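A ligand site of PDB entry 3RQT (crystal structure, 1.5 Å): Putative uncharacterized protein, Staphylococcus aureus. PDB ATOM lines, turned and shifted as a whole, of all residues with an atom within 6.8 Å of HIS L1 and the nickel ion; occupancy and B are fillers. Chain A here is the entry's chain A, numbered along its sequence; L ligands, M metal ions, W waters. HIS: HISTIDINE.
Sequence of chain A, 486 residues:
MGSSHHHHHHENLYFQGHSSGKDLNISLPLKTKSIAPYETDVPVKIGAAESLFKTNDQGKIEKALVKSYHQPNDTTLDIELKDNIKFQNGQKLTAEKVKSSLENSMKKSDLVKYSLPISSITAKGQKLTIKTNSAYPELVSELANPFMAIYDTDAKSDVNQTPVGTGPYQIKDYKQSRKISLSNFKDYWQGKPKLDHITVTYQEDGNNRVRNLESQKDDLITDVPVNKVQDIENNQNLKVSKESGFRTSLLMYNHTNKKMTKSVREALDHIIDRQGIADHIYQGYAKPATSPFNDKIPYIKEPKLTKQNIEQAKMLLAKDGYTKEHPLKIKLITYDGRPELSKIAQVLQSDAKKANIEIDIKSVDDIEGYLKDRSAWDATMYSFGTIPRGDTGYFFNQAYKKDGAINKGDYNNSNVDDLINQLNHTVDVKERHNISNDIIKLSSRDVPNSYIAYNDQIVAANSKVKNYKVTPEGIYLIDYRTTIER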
ATOM      1  N   LEU A  30      30.143  -5.130  -8.054  1.00  0.00           N
ATOM      2  CA  LEU A  30      28.795  -4.584  -8.244  1.00  0.00           C
ATOM      3  C   LEU A  30      27.687  -5.522  -7.863  1.00  0.00           C
ATOM      4  O   LEU A  30      26.825  -5.884  -8.680  1.00  0.00           O
ATOM      5  CB  LEU A  30      28.650  -3.995  -9.659  1.00  0.00           C
ATOM      6  CG  LEU A  30      29.705  -2.991 -10.071  1.00  0.00           C
ATOM      7  CD1 LEU A  30      29.363  -2.514 -11.508  1.00  0.00           C
ATOM      8  CD2 LEU A  30      29.850  -1.824  -9.101  1.00  0.00           C
ATOM      9  N   GLU A  39      16.614  -5.929 -14.029  1.00  0.00           N
ATOM     10  CA  GLU A  39      17.239  -5.184 -12.922  1.00  0.00           C
ATOM     11  C   GLU A  39      18.743  -5.049 -13.048  1.00  0.00           C
ATOM     12  O   GLU A  39      19.350  -4.177 -12.396  1.00  0.00           O
ATOM     13  CB  GLU A  39      16.923  -5.886 -11.604  1.00  0.00           C
ATOM     14  CG  GLU A  39      15.500  -5.765 -11.161  1.00  0.00           C
ATOM     15  CD  GLU A  39      15.102  -4.390 -10.700  1.00  0.00           C
ATOM     16  OE1 GLU A  39      15.968  -3.487 -10.503  1.00  0.00           O
ATOM     17  OE2 GLU A  39      13.889  -4.222 -10.498  1.00  0.00           O
ATOM     18  N   THR A  40      19.361  -5.945 -13.817  1.00  0.00           N
ATOM     19  CA  THR A  40      20.799  -6.007 -13.925  1.00  0.00           C
ATOM     20  C   THR A  40      21.216  -6.775 -15.167  1.00  0.00           C
ATOM     21  O   THR A  40      20.484  -7.683 -15.613  1.00  0.00           O
ATOM     22  CB  THR A  40      21.400  -6.723 -12.654  1.00  0.00           C
ATOM     23  OG1 THR A  40      22.760  -7.063 -12.852  1.00  0.00           O
ATOM     24  CG2 THR A  40      20.618  -8.024 -12.298  1.00  0.00           C
ATOM     25  N   ASP A  41      22.390  -6.436 -15.695  1.00  0.00           N
ATOM     26  CA  ASP A  41      22.941  -7.170 -16.837  1.00  0.00           C
ATOM     27  C   ASP A  41      23.691  -8.414 -16.429  1.00  0.00           C
ATOM     28  O   ASP A  41      24.221  -9.127 -17.274  1.00  0.00           O
ATOM     29  CB  ASP A  41      23.789  -6.243 -17.704  1.00  0.00           C
ATOM     30  CG  ASP A  41      25.078  -5.742 -17.045  1.00  0.00           C
ATOM     31  OD1 ASP A  41      25.474  -6.215 -15.936  1.00  0.00           O
ATOM     32  OD2 ASP A  41      25.741  -4.824 -17.642  1.00  0.00           O
ATOM     33  N   LEU A 111      14.119   1.700 -16.989  1.00  0.00           N
ATOM     34  CA  LEU A 111      15.175   1.627 -17.994  1.00  0.00           C
ATOM     35  C   LEU A 111      14.590   0.986 -19.233  1.00  0.00           C
ATOM     36  O   LEU A 111      14.680   1.537 -20.335  1.00  0.00           O
ATOM     37  CB  LEU A 111      16.386   0.849 -17.484  1.00  0.00           C
ATOM     38  CG  LEU A 111      17.596   0.763 -18.415  1.00  0.00           C
ATOM     39  CD1 LEU A 111      18.872   0.453 -17.601  1.00  0.00           C
ATOM     40  CD2 LEU A 111      17.442  -0.231 -19.531  1.00  0.00           C
ATOM     41  N   PRO A 146      20.998  -5.976 -22.617  1.00  0.00           N
ATOM     42  CA  PRO A 146      20.846  -7.119 -21.724  1.00  0.00           C
ATOM     43  C   PRO A 146      19.699  -6.992 -20.732  1.00  0.00           C
ATOM     44  O   PRO A 146      19.204  -7.985 -20.233  1.00  0.00           O
ATOM     45  CB  PRO A 146      22.208  -7.173 -21.023  1.00  0.00           C
ATOM     46  CG  PRO A 146      22.712  -5.773 -21.097  1.00  0.00           C
ATOM     47  CD  PRO A 146      22.332  -5.343 -22.479  1.00  0.00           C
ATOM     48  N   PHE A 147      19.244  -5.773 -20.451  1.00  0.00           N
ATOM     49  CA  PHE A 147      18.097  -5.548 -19.580  1.00  0.00           C
ATOM     50  C   PHE A 147      16.795  -6.050 -20.205  1.00  0.00           C
ATOM     51  O   PHE A 147      15.791  -6.192 -19.527  1.00  0.00           O
ATOM     52  CB  PHE A 147      17.950  -4.092 -19.135  1.00  0.00           C
ATOM     53  CG  PHE A 147      18.801  -3.717 -17.931  1.00  0.00           C
ATOM     54  CD1 PHE A 147      20.169  -3.726 -18.001  1.00  0.00           C
ATOM     55  CD2 PHE A 147      18.188  -3.267 -16.773  1.00  0.00           C
ATOM     56  CE1 PHE A 147      20.956  -3.322 -16.860  1.00  0.00           C
ATOM     57  CE2 PHE A 147      18.954  -2.861 -15.681  1.00  0.00           C
ATOM     58  CZ  PHE A 147      20.332  -2.898 -15.755  1.00  0.00           C
ATOM     59  N   ARG A 247      33.339   2.263 -22.082  1.00  0.00           N
ATOM     60  CA  ARG A 247      32.984   2.640 -20.730  1.00  0.00           C
ATOM     61  C   ARG A 247      33.688   3.947 -20.398  1.00  0.00           C
ATOM     62  O   ARG A 247      34.855   4.147 -20.739  1.00  0.00           O
ATOM     63  CB  ARG A 247      33.353   1.549 -19.735  1.00  0.00           C
ATOM     64  CG  ARG A 247      33.092   1.911 -18.287  1.00  0.00           C
ATOM     65  CD  ARG A 247      33.107   0.675 -17.421  1.00  0.00           C
ATOM     66  NE  ARG A 247      31.990  -0.203 -17.775  1.00  0.00           N
ATOM     67  CZ  ARG A 247      30.725   0.015 -17.413  1.00  0.00           C
ATOM     68  NH1 ARG A 247      30.403   1.055 -16.657  1.00  0.00           N
ATOM     69  NH2 ARG A 247      29.783  -0.823 -17.810  1.00  0.00           N
ATOM     70  N   TYR A 335      32.523   4.412  -4.811  1.00  0.00           N
ATOM     71  CA  TYR A 335      32.330   2.999  -4.592  1.00  0.00           C
ATOM     72  C   TYR A 335      33.542   2.251  -5.103  1.00  0.00           C
ATOM     73  O   TYR A 335      34.241   2.763  -5.980  1.00  0.00           O
ATOM     74  CB  TYR A 335      31.011   2.519  -5.217  1.00  0.00           C
ATOM     75  CG  TYR A 335      30.795   2.763  -6.705  1.00  0.00           C
ATOM     76  CD1 TYR A 335      30.899   1.712  -7.624  1.00  0.00           C
ATOM     77  CD2 TYR A 335      30.501   4.005  -7.203  1.00  0.00           C
ATOM     78  CE1 TYR A 335      30.679   1.935  -8.969  1.00  0.00           C
ATOM     79  CE2 TYR A 335      30.313   4.219  -8.541  1.00  0.00           C
ATOM     80  CZ  TYR A 335      30.431   3.197  -9.421  1.00  0.00           C
ATOM     81  OH  TYR A 335      30.212   3.430 -10.786  1.00  0.00           O
ATOM     82  N   ARG A 338      34.530  -0.304  -9.426  1.00  0.00           N
ATOM     83  CA  ARG A 338      35.382   0.156 -10.504  1.00  0.00           C
ATOM     84  C   ARG A 338      36.578   0.711  -9.726  1.00  0.00           C
ATOM     85  O   ARG A 338      36.485   1.804  -9.138  1.00  0.00           O
ATOM     86  CB  ARG A 338      34.703   1.218 -11.347  1.00  0.00           C
ATOM     87  CG  ARG A 338      33.313   0.873 -11.867  1.00  0.00           C
ATOM     88  CD  ARG A 338      33.320  -0.229 -12.873  1.00  0.00           C
ATOM     89  NE  ARG A 338      31.989  -0.437 -13.410  1.00  0.00           N
ATOM     90  CZ  ARG A 338      31.646  -1.454 -14.193  1.00  0.00           C
ATOM     91  NH1 ARG A 338      32.558  -2.339 -14.564  1.00  0.00           N
ATOM     92  NH2 ARG A 338      30.414  -1.584 -14.598  1.00  0.00           N
ATOM     93  N   GLU A 368      23.887   2.130  -6.528  1.00  0.00           N
ATOM     94  CA  GLU A 368      22.611   2.423  -7.181  1.00  0.00           C
ATOM     95  C   GLU A 368      21.556   2.704  -6.127  1.00  0.00           C
ATOM     96  O   GLU A 368      20.723   3.603  -6.291  1.00  0.00           O
ATOM     97  CB  GLU A 368      22.181   1.256  -8.084  1.00  0.00           C
ATOM     98  CG  GLU A 368      23.097   0.982  -9.269  1.00  0.00           C
ATOM     99  CD  GLU A 368      23.024   2.081 -10.282  1.00  0.00           C
ATOM    100  OE1 GLU A 368      22.134   2.002 -11.154  1.00  0.00           O
ATOM    101  OE2 GLU A 368      23.848   3.014 -10.202  1.00  0.00           O
ATOM    102  N   TYR A 382      31.147   7.957 -10.950  1.00  0.00           N
ATOM    103  CA  TYR A 382      30.277   7.020 -11.653  1.00  0.00           C
ATOM    104  C   TYR A 382      30.998   6.492 -12.888  1.00  0.00           C
ATOM    105  O   TYR A 382      31.986   7.046 -13.346  1.00  0.00           O
ATOM    106  CB  TYR A 382      28.946   7.705 -11.989  1.00  0.00           C
ATOM    107  CG  TYR A 382      27.762   6.776 -12.117  1.00  0.00           C
ATOM    108  CD1 TYR A 382      27.196   6.190 -10.967  1.00  0.00           C
ATOM    109  CD2 TYR A 382      27.203   6.461 -13.360  1.00  0.00           C
ATOM    110  CE1 TYR A 382      26.102   5.342 -11.079  1.00  0.00           C
ATOM    111  CE2 TYR A 382      26.122   5.604 -13.454  1.00  0.00           C
ATOM    112  CZ  TYR A 382      25.585   5.052 -12.313  1.00  0.00           C
ATOM    113  OH  TYR A 382      24.522   4.173 -12.437  1.00  0.00           O
ATOM    114  N   SER A 383      30.466   5.409 -13.413  1.00  0.00           N
ATOM    115  CA  SER A 383      30.984   4.774 -14.603  1.00  0.00           C
ATOM    116  C   SER A 383      29.832   4.191 -15.369  1.00  0.00           C
ATOM    117  O   SER A 383      28.947   3.585 -14.767  1.00  0.00           O
ATOM    118  CB  SER A 383      31.908   3.641 -14.180  1.00  0.00           C
ATOM    119  OG  SER A 383      32.362   2.885 -15.277  1.00  0.00           O
ATOM    120  N   PHE A 384      29.843   4.345 -16.682  1.00  0.00           N
ATOM    121  CA  PHE A 384      28.745   3.822 -17.466  1.00  0.00           C
ATOM    122  C   PHE A 384      29.200   3.426 -18.863  1.00  0.00           C
ATOM    123  O   PHE A 384      30.111   4.044 -19.418  1.00  0.00           O
ATOM    124  CB  PHE A 384      27.642   4.888 -17.592  1.00  0.00           C
ATOM    125  CG  PHE A 384      26.361   4.384 -18.197  1.00  0.00           C
ATOM    126  CD1 PHE A 384      25.607   3.431 -17.541  1.00  0.00           C
ATOM    127  CD2 PHE A 384      25.877   4.886 -19.376  1.00  0.00           C
ATOM    128  CE1 PHE A 384      24.410   2.985 -18.075  1.00  0.00           C
ATOM    129  CE2 PHE A 384      24.675   4.455 -19.893  1.00  0.00           C
ATOM    130  CZ  PHE A 384      23.952   3.471 -19.251  1.00  0.00           C
ATOM    131  N   GLY A 385      28.528   2.412 -19.411  1.00  0.00           N
ATOM    132  CA  GLY A 385      28.716   1.993 -20.800  1.00  0.00           C
ATOM    133  C   GLY A 385      27.869   2.941 -21.635  1.00  0.00           C
ATOM    134  O   GLY A 385      26.659   2.740 -21.796  1.00  0.00           O
ATOM    135  N   THR A 386      28.491   3.989 -22.157  1.00  0.00           N
ATOM    136  CA  THR A 386      27.751   5.049 -22.815  1.00  0.00           C
ATOM    137  C   THR A 386      27.300   4.801 -24.254  1.00  0.00           C
ATOM    138  O   THR A 386      26.474   5.542 -24.745  1.00  0.00           O
ATOM    139  CB  THR A 386      28.572   6.367 -22.785  1.00  0.00           C
ATOM    140  OG1 THR A 386      29.759   6.210 -23.557  1.00  0.00           O
ATOM    141  CG2 THR A 386      28.911   6.743 -21.320  1.00  0.00           C
ATOM    142  N   TYR A 394      20.677   5.999 -26.823  1.00  0.00           N
ATOM    143  CA  TYR A 394      20.444   5.300 -25.579  1.00  0.00           C
ATOM    144  C   TYR A 394      20.945   6.128 -24.399  1.00  0.00           C
ATOM    145  O   TYR A 394      20.214   6.366 -23.425  1.00  0.00           O
ATOM    146  CB  TYR A 394      21.147   3.935 -25.602  1.00  0.00           C
ATOM    147  CG  TYR A 394      21.018   3.174 -24.299  1.00  0.00           C
ATOM    148  CD1 TYR A 394      19.782   2.658 -23.897  1.00  0.00           C
ATOM    149  CD2 TYR A 394      22.115   2.911 -23.531  1.00  0.00           C
ATOM    150  CE1 TYR A 394      19.668   1.953 -22.736  1.00  0.00           C
ATOM    151  CE2 TYR A 394      22.001   2.170 -22.332  1.00  0.00           C
ATOM    152  CZ  TYR A 394      20.756   1.701 -21.967  1.00  0.00           C
ATOM    153  OH  TYR A 394      20.616   0.975 -20.802  1.00  0.00           O
ATOM    154  N   ALA A 405      16.929   6.146 -16.502  1.00  0.00           N
ATOM    155  CA  ALA A 405      17.425   5.274 -15.424  1.00  0.00           C
ATOM    156  C   ALA A 405      18.836   5.492 -14.939  1.00  0.00           C
ATOM    157  O   ALA A 405      19.206   4.943 -13.881  1.00  0.00           O
ATOM    158  CB  ALA A 405      17.182   3.834 -15.804  1.00  0.00           C
ATOM    159  N   ILE A 406      19.667   6.217 -15.665  1.00  0.00           N
ATOM    160  CA  ILE A 406      20.962   6.525 -15.043  1.00  0.00           C
ATOM    161  C   ILE A 406      21.099   8.006 -14.713  1.00  0.00           C
ATOM    162  O   ILE A 406      22.134   8.422 -14.219  1.00  0.00           O
ATOM    163  CB  ILE A 406      22.220   5.991 -15.783  1.00  0.00           C
ATOM    164  CG1 ILE A 406      22.553   6.824 -17.004  1.00  0.00           C
ATOM    165  CG2 ILE A 406      22.075   4.468 -16.080  1.00  0.00           C
ATOM    166  CD1 ILE A 406      23.974   6.766 -17.368  1.00  0.00           C
ATOM    167  N   LYS A 408      20.754   9.930 -12.335  1.00  0.00           N
ATOM    168  CA  LYS A 408      20.574   9.922 -10.895  1.00  0.00           C
ATOM    169  C   LYS A 408      20.520  11.326 -10.317  1.00  0.00           C
ATOM    170  O   LYS A 408      19.862  11.561  -9.317  1.00  0.00           O
ATOM    171  CB  LYS A 408      21.679   9.161 -10.164  1.00  0.00           C
ATOM    172  CG  LYS A 408      22.091   7.832 -10.747  1.00  0.00           C
ATOM    173  CD  LYS A 408      21.027   6.837 -10.812  1.00  0.00           C
ATOM    174  CE  LYS A 408      21.643   5.464 -11.253  1.00  0.00           C
ATOM    175  NZ  LYS A 408      20.631   4.410 -11.295  1.00  0.00           N
ATOM    176  N   GLU A 473      31.969  -3.650 -25.604  1.00  0.00           N
ATOM    177  CA  GLU A 473      30.771  -3.214 -24.884  1.00  0.00           C
ATOM    178  C   GLU A 473      30.850  -3.566 -23.378  1.00  0.00           C
ATOM    179  O   GLU A 473      30.152  -2.968 -22.555  1.00  0.00           O
ATOM    180  CB  GLU A 473      29.504  -3.815 -25.534  1.00  0.00           C
ATOM    181  CG  GLU A 473      29.134  -5.233 -25.072  1.00  0.00           C
ATOM    182  CD  GLU A 473      30.226  -6.300 -25.239  1.00  0.00           C
ATOM    183  OE1 GLU A 473      30.902  -6.339 -26.299  1.00  0.00           O
ATOM    184  OE2 GLU A 473      30.393  -7.127 -24.326  1.00  0.00           O
ATOM    185  N   ILE A 475      29.816  -6.124 -21.702  1.00  0.00           N
ATOM    186  CA  ILE A 475      28.640  -6.771 -21.132  1.00  0.00           C
ATOM    187  C   ILE A 475      28.818  -8.271 -21.087  1.00  0.00           C
ATOM    188  O   ILE A 475      28.614  -8.905 -20.039  1.00  0.00           O
ATOM    189  CB  ILE A 475      27.376  -6.406 -21.953  1.00  0.00           C
ATOM    190  CG1 ILE A 475      27.063  -4.904 -21.839  1.00  0.00           C
ATOM    191  CG2 ILE A 475      26.174  -7.274 -21.479  1.00  0.00           C
ATOM    192  CD1 ILE A 475      26.104  -4.344 -22.892  1.00  0.00           C
HETATM  193  N   HIS L   1      26.462  -1.676 -15.160  1.00  0.00           N
HETATM  194  CA  HIS L   1      26.126  -1.356 -16.568  1.00  0.00           C
HETATM  195  C   HIS L   1      26.756  -0.048 -16.992  1.00  0.00           C
HETATM  196  O   HIS L   1      27.147   0.763 -16.125  1.00  0.00           O
HETATM  197  CB  HIS L   1      24.598  -1.313 -16.756  1.00  0.00           C
HETATM  198  CG  HIS L   1      23.891  -0.307 -15.883  1.00  0.00           C
HETATM  199  ND1 HIS L   1      24.481   0.321 -14.793  1.00  0.00           N
HETATM  200  CD2 HIS L   1      22.590   0.052 -15.867  1.00  0.00           C
HETATM  201  CE1 HIS L   1      23.585   1.085 -14.197  1.00  0.00           C
HETATM  202  NE2 HIS L   1      22.422   0.935 -14.827  1.00  0.00           N
HETATM  203  OXT HIS L   1      26.940   0.198 -18.189  1.00  0.00           O
HETATM  204  N   HIS L   2      26.679   2.185 -13.500  1.00  0.00           N
HETATM  205  CA  HIS L   2      27.684   2.077 -12.390  1.00  0.00           C
HETATM  206  C   HIS L   2      28.766   1.127 -12.819  1.00  0.00           C
HETATM  207  O   HIS L   2      29.897   1.241 -12.332  1.00  0.00           O
HETATM  208  CB  HIS L   2      27.025   1.627 -11.081  1.00  0.00           C
HETATM  209  CG  HIS L   2      26.468   0.221 -11.097  1.00  0.00           C
HETATM  210  ND1 HIS L   2      26.009  -0.393 -12.239  1.00  0.00           N
HETATM  211  CD2 HIS L   2      26.213  -0.642 -10.071  1.00  0.00           C
HETATM  212  CE1 HIS L   2      25.528  -1.593 -11.927  1.00  0.00           C
HETATM  213  NE2 HIS L   2      25.606  -1.757 -10.614  1.00  0.00           N
HETATM  214  OXT HIS L   2      28.532   0.278 -13.667  1.00  0.00           O
HETATM  215 NI    NI M   1      26.449   0.231 -14.188  1.00  0.00          NI
HETATM  216  O   HOH W   1      26.756  -1.620 -20.207  1.00  0.00           O
HETATM  217  O   HOH W   2      19.860   2.006 -14.140  1.00  0.00           O
HETATM  218  O   HOH W   3      28.985  -3.982 -15.270  1.00  0.00           O
HETATM  219  O   HOH W   4      25.109   0.697 -20.991  1.00  0.00           O
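The backbone NH (N) of Ser 383 lies within hydrogen-bond range of the side-chain hydroxyl (OH) of Tyr 335, at 3.3 Å. The side-chain carboxylate (OE2) of Glu 368 sits at hydrogen-bond distance from the side-chain hydroxyl (OH) of Tyr 382, at 2.6 Å. The side-chain carboxylate (OE1) of Glu 368 lies within salt-bridge range of the side-chain amino group (NZ) of Lys 408, 2.8 Å away. The guanidinium group (NH1) of Arg 247 is in hydrogen-bond range of the side-chain hydroxyl (OG) of Ser 383.
No residue comes within 4 Å of the nickel ion.
Water W2 bridges NE2 of HIS L1 (2.9 Å) and O of Ala 405 (3.0 Å). Water W4 bridges the backbone carbonyl oxygen (O) of Gly 385 (2.7 Å) and an oxygen (OXT) of HIS L1 (3.4 Å).
Merely in contact with HIS L1: Asp 41, Phe 147, Arg 338, Glu 368, Tyr 382, Ser 383, Phe 384 and Ile 406. The nearest printed residue that does not touch HIS L1 is Leu 111 (4.1 Å).
The nickel ion is bound by ND1 of HIS L1 (2.1 Å), N of HIS L2 (2.1 Å), ND1 of HIS L2 (2.1 Å), O of HIS L1 (2.1 Å), N of HIS L1 (2.1 Å) and OXT of HIS L2 (2.1 Å).
An oxygen (OXT) of HIS L1 lies within salt-bridge range of the guanidinium group (NH2) of Arg 247 (3.0 Å). N of Gly 385 sits at hydrogen-bond distance from OXT of HIS L1 (3.0 Å). An oxygen (O) of HIS L2 lies within salt-bridge range of the guanidinium group (NE) of Arg 338. The side-chain hydroxyl (OH) of Tyr 335 is in hydrogen-bond range of an oxygen (O) of HIS L2 (2.7 Å). The guanidinium group of Arg 247 sits close to an oxygen (OXT) of HIS L2 (3.6 Å). A nitrogen (N) of HIS L2 lies close to the side-chain hydroxyl (OH) of Tyr 382. The backbone carbonyl oxygen of Ser 383 sits close to a nitrogen (N) of HIS L2 (3.0 Å).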
